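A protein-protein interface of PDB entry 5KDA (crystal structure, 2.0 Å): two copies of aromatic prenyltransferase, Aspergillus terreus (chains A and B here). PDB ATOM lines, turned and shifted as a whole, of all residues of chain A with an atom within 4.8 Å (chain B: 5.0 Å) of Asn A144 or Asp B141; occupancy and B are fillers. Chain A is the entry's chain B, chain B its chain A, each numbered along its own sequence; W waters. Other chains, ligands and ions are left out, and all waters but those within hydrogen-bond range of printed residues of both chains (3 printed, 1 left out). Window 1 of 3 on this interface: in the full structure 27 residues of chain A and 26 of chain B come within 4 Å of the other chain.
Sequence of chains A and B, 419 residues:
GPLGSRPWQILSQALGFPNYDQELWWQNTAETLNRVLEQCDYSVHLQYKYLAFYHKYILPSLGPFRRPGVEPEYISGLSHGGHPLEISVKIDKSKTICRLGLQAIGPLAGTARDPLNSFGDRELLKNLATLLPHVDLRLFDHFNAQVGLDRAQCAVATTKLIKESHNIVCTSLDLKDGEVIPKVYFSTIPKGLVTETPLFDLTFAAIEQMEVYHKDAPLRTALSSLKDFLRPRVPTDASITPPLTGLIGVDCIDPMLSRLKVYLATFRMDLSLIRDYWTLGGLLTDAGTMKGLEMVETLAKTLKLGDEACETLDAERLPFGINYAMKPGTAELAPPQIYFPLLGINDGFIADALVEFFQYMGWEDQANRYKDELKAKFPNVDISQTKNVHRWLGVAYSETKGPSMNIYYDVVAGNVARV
Among the printed residues, merely in contact across the chains: Asp A141 with Asp B141, His A142 with Ala B145, Ala A145 with Arg B138, Ala A145 with His B142 and Gln A146 with His B142.
The guanidinium group (NE) of Arg B122 lies within salt-bridge range of the side-chain carboxylate (OD1) of Asp B141, 2.8 Å away.
Water W2 lies within hydrogen-bond range of O of Ser A118 (2.6 Å), NH2 of Arg B122 (3.0 Å) and OD1 of Asn A144 (3.0 Å). Water W1 lies within hydrogen-bond range of the side-chain carboxylate (OD2) of Asp A141 (2.8 Å) and the backbone carbonyl oxygen (O) of Asn B144 (3.1 Å). Water W3 lies within hydrogen-bond range of OE1 of Gln A146 and ND1 of His B142.
Asp A141 touches its own counterpart, Asp B141. Asp A141 touches Asn B144, and with the chains exchanged Asn A144 touches Asp B141. His A142 touches Ala B145, and with the chains exchanged Ala A145 touches His B142. Positions printed for both chains: 140, 141, 142, 143, 144 and 145. Of the 9 pairs that touch across the chains among the printed residues, 5 have their exchanged pair printed and touching as well.
Printed residues of chain B that touch a printed residue of chain A: Arg B122, Arg B138, Asp B141, His B142, Asn B144 and Ala B145. Hydrophobic or aromatic side chains of chain B that line the printed part of chain A: His B142 and Ala B145.
Of the printed residues of chain B, His A142 touches Ala B145. Asn A144 touches just these residues of chain B: Arg B122 (3.3 Å) and Asp B141 (2.9 Å). Of the printed residues of chain B, Ala A145 touches Arg B138 and His B142. Phe A186 touches none of the printed residues of chain B. Leu B139 touches none of the printed residues of chain A. Asp B141 touches just these residues of chain A: Asp A141 (3.5 Å) and Asn A144 (2.9 Å). Printed residues of chain A within 4 Å of His B142: Ala A145 and Gln A146. The nearest residue of chain B that does not touch Asn A144 is Arg B138 (4.3 Å). The nearest residue of chain A that does not touch Asp B141 is Ala A145 (4.05 Å). The nearest printed residue of chain A that does not touch Arg B122 is Asp A141 (5.1 Å).
The guanidinium group of Arg B122 is in hydrogen-bond range of the side-chain amide oxygen of Asn A144. The guanidinium group (NH1) of Arg B138 is in hydrogen-bond range of the backbone carbonyl oxygen (O) of Gly A148 (3.5 Å). The side-chain carboxylate of Asp B141 lies close to the side-chain amide oxygen of Asn A144 (2.9 Å). ND2 of Asn B144 is in hydrogen-bond range of OD2 of Asp A141.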
ATOM      1  N   SER A 118     -17.123  13.904 -23.513  1.00  0.00           N
ATOM      2  CA  SER A 118     -18.389  14.226 -24.243  1.00  0.00           C
ATOM      3  C   SER A 118     -18.517  13.760 -25.701  1.00  0.00           C
ATOM      4  O   SER A 118     -19.599  13.798 -26.249  1.00  0.00           O
ATOM      5  CB  SER A 118     -18.639  15.736 -24.190  1.00  0.00           C
ATOM      6  OG  SER A 118     -18.993  16.119 -22.880  1.00  0.00           O
ATOM      7  N   PHE A 140     -29.849   8.922 -29.784  1.00  0.00           N
ATOM      8  CA  PHE A 140     -28.618   9.414 -29.243  1.00  0.00           C
ATOM      9  C   PHE A 140     -28.607  10.911 -29.286  1.00  0.00           C
ATOM     10  O   PHE A 140     -28.299  11.567 -28.285  1.00  0.00           O
ATOM     11  CB  PHE A 140     -27.391   8.886 -29.996  1.00  0.00           C
ATOM     12  CG  PHE A 140     -26.124   9.248 -29.346  1.00  0.00           C
ATOM     13  CD1 PHE A 140     -25.545  10.533 -29.509  1.00  0.00           C
ATOM     14  CD2 PHE A 140     -25.501   8.351 -28.494  1.00  0.00           C
ATOM     15  CE1 PHE A 140     -24.404  10.887 -28.855  1.00  0.00           C
ATOM     16  CE2 PHE A 140     -24.344   8.714 -27.839  1.00  0.00           C
ATOM     17  CZ  PHE A 140     -23.800   9.959 -28.006  1.00  0.00           C
ATOM     18  N   ASP A 141     -28.797  11.470 -30.491  1.00  0.00           N
ATOM     19  CA  ASP A 141     -28.617  12.865 -30.664  1.00  0.00           C
ATOM     20  C   ASP A 141     -29.689  13.640 -29.822  1.00  0.00           C
ATOM     21  O   ASP A 141     -29.377  14.631 -29.210  1.00  0.00           O
ATOM     22  CB  ASP A 141     -28.660  13.223 -32.105  1.00  0.00           C
ATOM     23  CG  ASP A 141     -27.365  12.834 -32.853  1.00  0.00           C
ATOM     24  OD1 ASP A 141     -26.318  12.534 -32.215  1.00  0.00           O
ATOM     25  OD2 ASP A 141     -27.402  12.882 -34.118  1.00  0.00           O
ATOM     26  N   HIS A 142     -30.900  13.133 -29.775  1.00  0.00           N
ATOM     27  CA  HIS A 142     -31.941  13.720 -28.953  1.00  0.00           C
ATOM     28  C   HIS A 142     -31.487  13.831 -27.494  1.00  0.00           C
ATOM     29  O   HIS A 142     -31.468  14.912 -26.950  1.00  0.00           O
ATOM     30  CB  HIS A 142     -33.272  12.937 -29.052  1.00  0.00           C
ATOM     31  CG  HIS A 142     -34.304  13.468 -28.085  1.00  0.00           C
ATOM     32  ND1 HIS A 142     -34.950  14.656 -28.294  1.00  0.00           N
ATOM     33  CD2 HIS A 142     -34.595  13.104 -26.813  1.00  0.00           C
ATOM     34  CE1 HIS A 142     -35.703  14.938 -27.242  1.00  0.00           C
ATOM     35  NE2 HIS A 142     -35.494  14.020 -26.325  1.00  0.00           N
ATOM     36  N   PHE A 143     -31.066  12.726 -26.857  1.00  0.00           N
ATOM     37  CA  PHE A 143     -30.720  12.793 -25.434  1.00  0.00           C
ATOM     38  C   PHE A 143     -29.378  13.495 -25.153  1.00  0.00           C
ATOM     39  O   PHE A 143     -29.242  14.113 -24.129  1.00  0.00           O
ATOM     40  CB  PHE A 143     -30.824  11.411 -24.823  1.00  0.00           C
ATOM     41  CG  PHE A 143     -32.254  11.024 -24.530  1.00  0.00           C
ATOM     42  CD1 PHE A 143     -32.946  11.666 -23.459  1.00  0.00           C
ATOM     43  CD2 PHE A 143     -32.904  10.125 -25.294  1.00  0.00           C
ATOM     44  CE1 PHE A 143     -34.253  11.370 -23.186  1.00  0.00           C
ATOM     45  CE2 PHE A 143     -34.258   9.815 -25.043  1.00  0.00           C
ATOM     46  CZ  PHE A 143     -34.917  10.439 -23.978  1.00  0.00           C
ATOM     47  N   ASN A 144     -28.417  13.431 -26.073  1.00  0.00           N
ATOM     48  CA  ASN A 144     -27.166  14.202 -25.997  1.00  0.00           C
ATOM     49  C   ASN A 144     -27.514  15.731 -26.035  1.00  0.00           C
ATOM     50  O   ASN A 144     -26.890  16.522 -25.377  1.00  0.00           O
ATOM     51  CB  ASN A 144     -26.189  13.823 -27.142  1.00  0.00           C
ATOM     52  CG  ASN A 144     -24.771  14.270 -26.890  1.00  0.00           C
ATOM     53  OD1 ASN A 144     -24.044  14.775 -27.808  1.00  0.00           O
ATOM     54  ND2 ASN A 144     -24.335  14.071 -25.672  1.00  0.00           N
ATOM     55  N   ALA A 145     -28.543  16.122 -26.771  1.00  0.00           N
ATOM     56  CA  ALA A 145     -28.996  17.506 -26.748  1.00  0.00           C
ATOM     57  C   ALA A 145     -29.609  17.917 -25.408  1.00  0.00           C
ATOM     58  O   ALA A 145     -29.435  19.053 -24.997  1.00  0.00           O
ATOM     59  CB  ALA A 145     -29.992  17.755 -27.878  1.00  0.00           C
ATOM     60  N   GLN A 146     -30.316  17.010 -24.756  1.00  0.00           N
ATOM     61  CA  GLN A 146     -31.070  17.350 -23.567  1.00  0.00           C
ATOM     62  C   GLN A 146     -30.244  17.179 -22.326  1.00  0.00           C
ATOM     63  O   GLN A 146     -30.452  17.905 -21.375  1.00  0.00           O
ATOM     64  CB  GLN A 146     -32.324  16.491 -23.448  1.00  0.00           C
ATOM     65  CG  GLN A 146     -33.143  16.331 -24.716  1.00  0.00           C
ATOM     66  CD  GLN A 146     -33.713  17.628 -25.232  1.00  0.00           C
ATOM     67  OE1 GLN A 146     -33.758  17.903 -26.472  1.00  0.00           O
ATOM     68  NE2 GLN A 146     -34.201  18.421 -24.290  1.00  0.00           N
ATOM     69  N   VAL A 147     -29.283  16.259 -22.283  1.00  0.00           N
ATOM     70  CA  VAL A 147     -28.481  16.187 -21.066  1.00  0.00           C
ATOM     71  C   VAL A 147     -26.995  16.455 -21.207  1.00  0.00           C
ATOM     72  O   VAL A 147     -26.218  16.415 -20.199  1.00  0.00           O
ATOM     73  CB  VAL A 147     -28.766  14.893 -20.286  1.00  0.00           C
ATOM     74  CG1 VAL A 147     -30.253  14.868 -19.887  1.00  0.00           C
ATOM     75  CG2 VAL A 147     -28.398  13.660 -21.074  1.00  0.00           C
ATOM     76  N   GLY A 148     -26.567  16.721 -22.436  1.00  0.00           N
ATOM     77  CA  GLY A 148     -25.185  17.110 -22.650  1.00  0.00           C
ATOM     78  C   GLY A 148     -24.944  18.477 -22.059  1.00  0.00           C
ATOM     79  O   GLY A 148     -25.892  19.187 -21.758  1.00  0.00           O
ATOM     80  N   PHE A 186     -27.428   7.649 -20.870  1.00  0.00           N
ATOM     81  CA  PHE A 186     -27.025   9.011 -20.585  1.00  0.00           C
ATOM     82  C   PHE A 186     -27.257   9.251 -19.141  1.00  0.00           C
ATOM     83  O   PHE A 186     -28.327   8.921 -18.611  1.00  0.00           O
ATOM     84  CB  PHE A 186     -27.849  10.015 -21.392  1.00  0.00           C
ATOM     85  CG  PHE A 186     -27.538  10.011 -22.870  1.00  0.00           C
ATOM     86  CD1 PHE A 186     -28.229   9.233 -23.724  1.00  0.00           C
ATOM     87  CD2 PHE A 186     -26.546  10.839 -23.378  1.00  0.00           C
ATOM     88  CE1 PHE A 186     -27.916   9.226 -25.064  1.00  0.00           C
ATOM     89  CE2 PHE A 186     -26.262  10.850 -24.730  1.00  0.00           C
ATOM     90  CZ  PHE A 186     -26.926  10.024 -25.558  1.00  0.00           C
ATOM     91  N   ARG B 122     -20.892  17.056 -38.347  1.00  0.00           N
ATOM     92  CA  ARG B 122     -20.805  16.800 -36.872  1.00  0.00           C
ATOM     93  C   ARG B 122     -19.387  16.428 -36.418  1.00  0.00           C
ATOM     94  O   ARG B 122     -18.935  16.874 -35.376  1.00  0.00           O
ATOM     95  CB  ARG B 122     -21.861  15.763 -36.461  1.00  0.00           C
ATOM     96  CG  ARG B 122     -21.873  15.261 -35.034  1.00  0.00           C
ATOM     97  CD  ARG B 122     -22.187  16.357 -34.093  1.00  0.00           C
ATOM     98  NE  ARG B 122     -22.628  15.956 -32.724  1.00  0.00           N
ATOM     99  CZ  ARG B 122     -21.812  15.521 -31.761  1.00  0.00           C
ATOM    100  NH1 ARG B 122     -20.514  15.307 -31.997  1.00  0.00           N
ATOM    101  NH2 ARG B 122     -22.280  15.352 -30.554  1.00  0.00           N
ATOM    102  N   LEU B 137     -22.666  22.058 -28.980  1.00  0.00           N
ATOM    103  CA  LEU B 137     -23.275  21.092 -29.946  1.00  0.00           C
ATOM    104  C   LEU B 137     -24.733  20.754 -29.686  1.00  0.00           C
ATOM    105  O   LEU B 137     -25.314  19.920 -30.388  1.00  0.00           O
ATOM    106  CB  LEU B 137     -22.519  19.788 -29.888  1.00  0.00           C
ATOM    107  CG  LEU B 137     -21.020  19.757 -30.237  1.00  0.00           C
ATOM    108  CD1 LEU B 137     -20.778  18.468 -30.986  1.00  0.00           C
ATOM    109  CD2 LEU B 137     -20.475  20.887 -31.075  1.00  0.00           C
ATOM    110  N   ARG B 138     -25.356  21.393 -28.707  1.00  0.00           N
ATOM    111  CA  ARG B 138     -26.671  20.896 -28.295  1.00  0.00           C
ATOM    112  C   ARG B 138     -27.736  21.184 -29.272  1.00  0.00           C
ATOM    113  O   ARG B 138     -28.571  20.345 -29.522  1.00  0.00           O
ATOM    114  CB  ARG B 138     -27.050  21.373 -26.916  1.00  0.00           C
ATOM    115  CG  ARG B 138     -26.189  20.688 -25.869  1.00  0.00           C
ATOM    116  CD  ARG B 138     -26.426  21.301 -24.515  1.00  0.00           C
ATOM    117  NE  ARG B 138     -25.803  22.620 -24.390  1.00  0.00           N
ATOM    118  CZ  ARG B 138     -25.546  23.217 -23.223  1.00  0.00           C
ATOM    119  NH1 ARG B 138     -25.887  22.667 -22.073  1.00  0.00           N
ATOM    120  NH2 ARG B 138     -24.985  24.376 -23.205  1.00  0.00           N
ATOM    121  N   LEU B 139     -27.689  22.348 -29.899  1.00  0.00           N
ATOM    122  CA  LEU B 139     -28.677  22.646 -30.895  1.00  0.00           C
ATOM    123  C   LEU B 139     -28.455  21.873 -32.183  1.00  0.00           C
ATOM    124  O   LEU B 139     -29.444  21.419 -32.812  1.00  0.00           O
ATOM    125  CB  LEU B 139     -28.765  24.148 -31.118  1.00  0.00           C
ATOM    126  CG  LEU B 139     -29.494  24.926 -30.019  1.00  0.00           C
ATOM    127  CD1 LEU B 139     -29.564  26.425 -30.298  1.00  0.00           C
ATOM    128  CD2 LEU B 139     -30.888  24.411 -29.880  1.00  0.00           C
ATOM    129  N   PHE B 140     -27.217  21.753 -32.628  1.00  0.00           N
ATOM    130  CA  PHE B 140     -26.907  20.851 -33.709  1.00  0.00           C
ATOM    131  C   PHE B 140     -27.576  19.474 -33.481  1.00  0.00           C
ATOM    132  O   PHE B 140     -28.349  19.011 -34.309  1.00  0.00           O
ATOM    133  CB  PHE B 140     -25.422  20.702 -33.945  1.00  0.00           C
ATOM    134  CG  PHE B 140     -25.107  19.780 -35.119  1.00  0.00           C
ATOM    135  CD1 PHE B 140     -25.266  18.417 -35.016  1.00  0.00           C
ATOM    136  CD2 PHE B 140     -24.678  20.293 -36.314  1.00  0.00           C
ATOM    137  CE1 PHE B 140     -25.044  17.581 -36.084  1.00  0.00           C
ATOM    138  CE2 PHE B 140     -24.362  19.459 -37.375  1.00  0.00           C
ATOM    139  CZ  PHE B 140     -24.562  18.107 -37.267  1.00  0.00           C
ATOM    140  N   ASP B 141     -27.284  18.846 -32.367  1.00  0.00           N
ATOM    141  CA  ASP B 141     -27.807  17.524 -32.078  1.00  0.00           C
ATOM    142  C   ASP B 141     -29.326  17.439 -32.008  1.00  0.00           C
ATOM    143  O   ASP B 141     -29.946  16.463 -32.384  1.00  0.00           O
ATOM    144  CB  ASP B 141     -27.226  17.041 -30.746  1.00  0.00           C
ATOM    145  CG  ASP B 141     -25.739  16.648 -30.849  1.00  0.00           C
ATOM    146  OD1 ASP B 141     -25.282  16.401 -31.967  1.00  0.00           O
ATOM    147  OD2 ASP B 141     -24.986  16.623 -29.819  1.00  0.00           O
ATOM    148  N   HIS B 142     -29.934  18.481 -31.468  1.00  0.00           N
ATOM    149  CA  HIS B 142     -31.369  18.522 -31.444  1.00  0.00           C
ATOM    150  C   HIS B 142     -31.950  18.447 -32.849  1.00  0.00           C
ATOM    151  O   HIS B 142     -32.874  17.649 -33.103  1.00  0.00           O
ATOM    152  CB  HIS B 142     -31.857  19.810 -30.773  1.00  0.00           C
ATOM    153  CG  HIS B 142     -33.315  19.958 -30.875  1.00  0.00           C
ATOM    154  ND1 HIS B 142     -34.170  19.227 -30.092  1.00  0.00           N
ATOM    155  CD2 HIS B 142     -34.083  20.650 -31.748  1.00  0.00           C
ATOM    156  CE1 HIS B 142     -35.407  19.532 -30.422  1.00  0.00           C
ATOM    157  NE2 HIS B 142     -35.382  20.389 -31.428  1.00  0.00           N
ATOM    158  N   PHE B 143     -31.500  19.311 -33.739  1.00  0.00           N
ATOM    159  CA  PHE B 143     -32.042  19.335 -35.088  1.00  0.00           C
ATOM    160  C   PHE B 143     -31.617  18.100 -35.947  1.00  0.00           C
ATOM    161  O   PHE B 143     -32.408  17.565 -36.775  1.00  0.00           O
ATOM    162  CB  PHE B 143     -31.769  20.666 -35.767  1.00  0.00           C
ATOM    163  CG  PHE B 143     -32.677  21.758 -35.271  1.00  0.00           C
ATOM    164  CD1 PHE B 143     -34.021  21.728 -35.575  1.00  0.00           C
ATOM    165  CD2 PHE B 143     -32.223  22.686 -34.368  1.00  0.00           C
ATOM    166  CE1 PHE B 143     -34.917  22.692 -35.066  1.00  0.00           C
ATOM    167  CE2 PHE B 143     -33.104  23.644 -33.847  1.00  0.00           C
ATOM    168  CZ  PHE B 143     -34.419  23.656 -34.204  1.00  0.00           C
ATOM    169  N   ASN B 144     -30.422  17.626 -35.734  1.00  0.00           N
ATOM    170  CA  ASN B 144     -29.997  16.373 -36.378  1.00  0.00           C
ATOM    171  C   ASN B 144     -30.957  15.263 -35.941  1.00  0.00           C
ATOM    172  O   ASN B 144     -31.352  14.446 -36.749  1.00  0.00           O
ATOM    173  CB  ASN B 144     -28.565  16.057 -36.013  1.00  0.00           C
ATOM    174  CG  ASN B 144     -27.854  15.227 -37.083  1.00  0.00           C
ATOM    175  OD1 ASN B 144     -28.073  15.362 -38.311  1.00  0.00           O
ATOM    176  ND2 ASN B 144     -26.974  14.374 -36.611  1.00  0.00           N
ATOM    177  N   ALA B 145     -31.382  15.259 -34.672  1.00  0.00           N
ATOM    178  CA  ALA B 145     -32.362  14.300 -34.217  1.00  0.00           C
ATOM    179  C   ALA B 145     -33.669  14.433 -34.928  1.00  0.00           C
ATOM    180  O   ALA B 145     -34.274  13.410 -35.235  1.00  0.00           O
ATOM    181  CB  ALA B 145     -32.647  14.434 -32.715  1.00  0.00           C
HETATM  182  O   HOH W   1     -29.792  12.152 -35.451  1.00  0.00           O
HETATM  183  O   HOH W   2     -21.045  15.317 -27.797  1.00  0.00           O
HETATM  184  O   HOH W   3     -33.373  20.806 -27.393  1.00  0.00           O
